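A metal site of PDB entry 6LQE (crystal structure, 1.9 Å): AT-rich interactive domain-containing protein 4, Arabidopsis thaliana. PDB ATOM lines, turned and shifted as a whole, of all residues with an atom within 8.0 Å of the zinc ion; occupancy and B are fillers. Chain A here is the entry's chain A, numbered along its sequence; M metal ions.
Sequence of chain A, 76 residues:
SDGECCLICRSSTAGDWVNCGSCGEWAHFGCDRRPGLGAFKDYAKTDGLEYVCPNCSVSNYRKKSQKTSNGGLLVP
SG of Cys 56 lies close to OG of Ser 22 (3.5 Å). SG of Cys 53 sits close to N of Asn 55, 3.8 Å away. The backbone carbonyl oxygen of Cys 53 lies within hydrogen-bond range of the side-chain hydroxyl of Ser 57 (3.0 Å). The side-chain sulfur (SG) of Cys 23 sits close to the backbone NH (N) of Glu 25. The side-chain sulfur (SG) of Cys 20 lies close to the backbone NH (N) of Ser 22 (3.2 Å). The backbone carbonyl oxygen of Glu 25 is in hydrogen-bond range of the backbone NH of Cys 20.
Within 4 Å of the zinc ion: Cys 20, Cys 23, Cys 53 and Cys 56.
The zinc ion is bound by SG of Cys 56 (2.2 Å), SG of Cys 53 (2.3 Å), SG of Cys 23 (2.5 Å) and SG of Cys 20 (2.5 Å).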
ATOM      1  N   LEU A   7      15.545  18.731   6.815  1.00  0.00           N
ATOM      2  CA  LEU A   7      14.951  18.182   8.033  1.00  0.00           C
ATOM      3  C   LEU A   7      14.285  16.835   7.756  1.00  0.00           C
ATOM      4  O   LEU A   7      13.980  16.095   8.691  1.00  0.00           O
ATOM      5  CB  LEU A   7      13.942  19.193   8.644  1.00  0.00           C
ATOM      6  CG  LEU A   7      12.653  19.540   7.887  1.00  0.00           C
ATOM      7  CD1 LEU A   7      11.529  18.624   8.284  1.00  0.00           C
ATOM      8  CD2 LEU A   7      12.231  20.990   8.123  1.00  0.00           C
ATOM      9  N   ASN A  19      12.040  26.978   4.076  1.00  0.00           N
ATOM     10  CA  ASN A  19      12.309  27.119   5.498  1.00  0.00           C
ATOM     11  C   ASN A  19      11.010  27.028   6.285  1.00  0.00           C
ATOM     12  O   ASN A  19      10.006  27.655   5.926  1.00  0.00           O
ATOM     13  CB  ASN A  19      13.023  28.444   5.790  1.00  0.00           C
ATOM     14  CG  ASN A  19      13.402  28.592   7.250  1.00  0.00           C
ATOM     15  OD1 ASN A  19      12.746  29.290   8.025  1.00  0.00           O
ATOM     16  ND2 ASN A  19      14.477  27.940   7.634  1.00  0.00           N
ATOM     17  N   CYS A  20      11.000  26.228   7.346  1.00  0.00           N
ATOM     18  CA  CYS A  20       9.800  26.125   8.142  1.00  0.00           C
ATOM     19  C   CYS A  20       9.589  27.405   8.919  1.00  0.00           C
ATOM     20  O   CYS A  20      10.539  27.958   9.481  1.00  0.00           O
ATOM     21  CB  CYS A  20       9.872  24.942   9.098  1.00  0.00           C
ATOM     22  SG  CYS A  20       8.384  24.798  10.083  1.00  0.00           S
ATOM     23  N   GLY A  21       8.358  27.896   8.940  1.00  0.00           N
ATOM     24  CA  GLY A  21       8.053  29.118   9.662  1.00  0.00           C
ATOM     25  C   GLY A  21       7.788  28.889  11.135  1.00  0.00           C
ATOM     26  O   GLY A  21       7.611  29.840  11.900  1.00  0.00           O
ATOM     27  N   SER A  22       7.761  27.633  11.540  1.00  0.00           N
ATOM     28  CA  SER A  22       7.525  27.308  12.936  1.00  0.00           C
ATOM     29  C   SER A  22       8.844  27.031  13.655  1.00  0.00           C
ATOM     30  O   SER A  22       9.160  27.656  14.659  1.00  0.00           O
ATOM     31  CB  SER A  22       6.588  26.107  13.065  1.00  0.00           C
ATOM     32  OG  SER A  22       6.423  25.732  14.424  1.00  0.00           O
ATOM     33  N   CYS A  23       9.604  26.090  13.104  1.00  0.00           N
ATOM     34  CA  CYS A  23      10.837  25.644  13.760  1.00  0.00           C
ATOM     35  C   CYS A  23      12.080  26.279  13.158  1.00  0.00           C
ATOM     36  O   CYS A  23      13.142  26.262  13.772  1.00  0.00           O
ATOM     37  CB  CYS A  23      10.940  24.123  13.679  1.00  0.00           C
ATOM     38  SG  CYS A  23      11.301  23.464  12.035  1.00  0.00           S
ATOM     39  N   GLY A  24      11.962  26.829  11.959  1.00  0.00           N
ATOM     40  CA  GLY A  24      13.100  27.507  11.338  1.00  0.00           C
ATOM     41  C   GLY A  24      14.144  26.588  10.719  1.00  0.00           C
ATOM     42  O   GLY A  24      15.199  27.056  10.264  1.00  0.00           O
ATOM     43  N   GLU A  25      13.864  25.281  10.682  1.00  0.00           N
ATOM     44  CA  GLU A  25      14.721  24.340   9.953  1.00  0.00           C
ATOM     45  C   GLU A  25      14.402  24.364   8.462  1.00  0.00           C
ATOM     46  O   GLU A  25      13.321  24.811   8.056  1.00  0.00           O
ATOM     47  CB  GLU A  25      14.538  22.933  10.511  1.00  0.00           C
ATOM     48  CG  GLU A  25      14.837  22.827  11.994  1.00  0.00           C
ATOM     49  CD  GLU A  25      14.892  21.380  12.460  1.00  0.00           C
ATOM     50  OE1 GLU A  25      15.604  20.574  11.818  1.00  0.00           O
ATOM     51  OE2 GLU A  25      14.220  21.055  13.459  1.00  0.00           O
ATOM     52  N   TRP A  26      15.332  23.881   7.635  1.00  0.00           N
ATOM     53  CA  TRP A  26      15.143  23.817   6.179  1.00  0.00           C
ATOM     54  C   TRP A  26      14.770  22.420   5.692  1.00  0.00           C
ATOM     55  O   TRP A  26      15.079  21.435   6.345  1.00  0.00           O
ATOM     56  CB  TRP A  26      16.412  24.253   5.453  1.00  0.00           C
ATOM     57  CG  TRP A  26      16.732  25.707   5.555  1.00  0.00           C
ATOM     58  CD1 TRP A  26      17.523  26.305   6.490  1.00  0.00           C
ATOM     59  CD2 TRP A  26      16.308  26.740   4.661  1.00  0.00           C
ATOM     60  NE1 TRP A  26      17.609  27.652   6.237  1.00  0.00           N
ATOM     61  CE2 TRP A  26      16.871  27.940   5.125  1.00  0.00           C
ATOM     62  CE3 TRP A  26      15.503  26.771   3.528  1.00  0.00           C
ATOM     63  CZ2 TRP A  26      16.641  29.164   4.488  1.00  0.00           C
ATOM     64  CZ3 TRP A  26      15.286  27.975   2.894  1.00  0.00           C
ATOM     65  CH2 TRP A  26      15.853  29.156   3.373  1.00  0.00           C
ATOM     66  N   ARG A  34       3.460  15.510   1.195  1.00  0.00           N
ATOM     67  CA  ARG A  34       2.096  15.666   1.686  1.00  0.00           C
ATOM     68  C   ARG A  34       1.142  16.172   0.583  1.00  0.00           C
ATOM     69  O   ARG A  34       1.476  17.086  -0.149  1.00  0.00           O
ATOM     70  CB  ARG A  34       2.059  16.629   2.876  1.00  0.00           C
ATOM     71  CG  ARG A  34       2.630  16.035   4.147  1.00  0.00           C
ATOM     72  CD  ARG A  34       2.600  17.030   5.274  1.00  0.00           C
ATOM     73  NE  ARG A  34       3.531  18.138   5.047  1.00  0.00           N
ATOM     74  CZ  ARG A  34       3.591  19.225   5.795  1.00  0.00           C
ATOM     75  NH1 ARG A  34       2.762  19.379   6.825  1.00  0.00           N
ATOM     76  NH2 ARG A  34       4.477  20.171   5.518  1.00  0.00           N
ATOM     77  N   TYR A  51       5.530  27.965   4.637  1.00  0.00           N
ATOM     78  CA  TYR A  51       5.785  26.547   4.758  1.00  0.00           C
ATOM     79  C   TYR A  51       5.881  26.144   6.211  1.00  0.00           C
ATOM     80  O   TYR A  51       6.623  26.764   6.972  1.00  0.00           O
ATOM     81  CB  TYR A  51       7.069  26.151   4.028  1.00  0.00           C
ATOM     82  CG  TYR A  51       7.407  24.684   4.187  1.00  0.00           C
ATOM     83  CD1 TYR A  51       6.659  23.711   3.533  1.00  0.00           C
ATOM     84  CD2 TYR A  51       8.464  24.271   4.987  1.00  0.00           C
ATOM     85  CE1 TYR A  51       6.961  22.379   3.676  1.00  0.00           C
ATOM     86  CE2 TYR A  51       8.761  22.930   5.128  1.00  0.00           C
ATOM     87  CZ  TYR A  51       8.010  21.995   4.476  1.00  0.00           C
ATOM     88  OH  TYR A  51       8.309  20.675   4.624  1.00  0.00           O
ATOM     89  N   VAL A  52       5.125  25.131   6.596  1.00  0.00           N
ATOM     90  CA  VAL A  52       5.235  24.567   7.938  1.00  0.00           C
ATOM     91  C   VAL A  52       5.493  23.091   7.762  1.00  0.00           C
ATOM     92  O   VAL A  52       4.674  22.382   7.158  1.00  0.00           O
ATOM     93  CB  VAL A  52       3.962  24.840   8.783  1.00  0.00           C
ATOM     94  CG1 VAL A  52       4.078  24.230  10.173  1.00  0.00           C
ATOM     95  CG2 VAL A  52       3.714  26.314   8.885  1.00  0.00           C
ATOM     96  N   CYS A  53       6.649  22.628   8.259  1.00  0.00           N
ATOM     97  CA  CYS A  53       7.122  21.265   8.067  1.00  0.00           C
ATOM     98  C   CYS A  53       6.164  20.231   8.682  1.00  0.00           C
ATOM     99  O   CYS A  53       5.280  20.595   9.467  1.00  0.00           O
ATOM    100  CB  CYS A  53       8.538  21.127   8.659  1.00  0.00           C
ATOM    101  SG  CYS A  53       8.604  20.813  10.431  1.00  0.00           S
ATOM    102  N   PRO A  54       6.308  18.946   8.305  1.00  0.00           N
ATOM    103  CA  PRO A  54       5.358  17.915   8.741  1.00  0.00           C
ATOM    104  C   PRO A  54       5.229  17.787  10.254  1.00  0.00           C
ATOM    105  O   PRO A  54       4.105  17.674  10.773  1.00  0.00           O
ATOM    106  CB  PRO A  54       5.946  16.658   8.133  1.00  0.00           C
ATOM    107  CG  PRO A  54       6.530  17.156   6.874  1.00  0.00           C
ATOM    108  CD  PRO A  54       7.208  18.424   7.272  1.00  0.00           C
ATOM    109  N   ASN A  55       6.349  17.808  10.969  1.00  0.00           N
ATOM    110  CA  ASN A  55       6.255  17.722  12.415  1.00  0.00           C
ATOM    111  C   ASN A  55       5.602  18.931  13.056  1.00  0.00           C
ATOM    112  O   ASN A  55       4.817  18.778  13.997  1.00  0.00           O
ATOM    113  CB  ASN A  55       7.631  17.498  13.038  1.00  0.00           C
ATOM    114  CG  ASN A  55       7.983  16.033  13.135  1.00  0.00           C
ATOM    115  OD1 ASN A  55       9.081  15.623  12.787  1.00  0.00           O
ATOM    116  ND2 ASN A  55       7.010  15.224  13.565  1.00  0.00           N
ATOM    117  N   CYS A  56       5.888  20.125  12.552  1.00  0.00           N
ATOM    118  CA  CYS A  56       5.312  21.341  13.155  1.00  0.00           C
ATOM    119  C   CYS A  56       3.839  21.537  12.816  1.00  0.00           C
ATOM    120  O   CYS A  56       3.123  22.277  13.509  1.00  0.00           O
ATOM    121  CB  CYS A  56       6.108  22.576  12.736  1.00  0.00           C
ATOM    122  SG  CYS A  56       7.790  22.656  13.373  1.00  0.00           S
ATOM    123  N   SER A  57       3.366  20.886  11.766  1.00  0.00           N
ATOM    124  CA  SER A  57       1.999  21.098  11.320  1.00  0.00           C
ATOM    125  C   SER A  57       0.976  20.566  12.339  1.00  0.00           C
ATOM    126  O   SER A  57       0.180  21.362  12.846  1.00  0.00           O
ATOM    127  CB  SER A  57       1.806  20.474   9.937  1.00  0.00           C
ATOM    128  OG  SER A  57       2.424  21.285   8.953  1.00  0.00           O
HETATM  129 ZN    ZN M   1       8.969  22.800  11.484  1.00  0.00          ZN
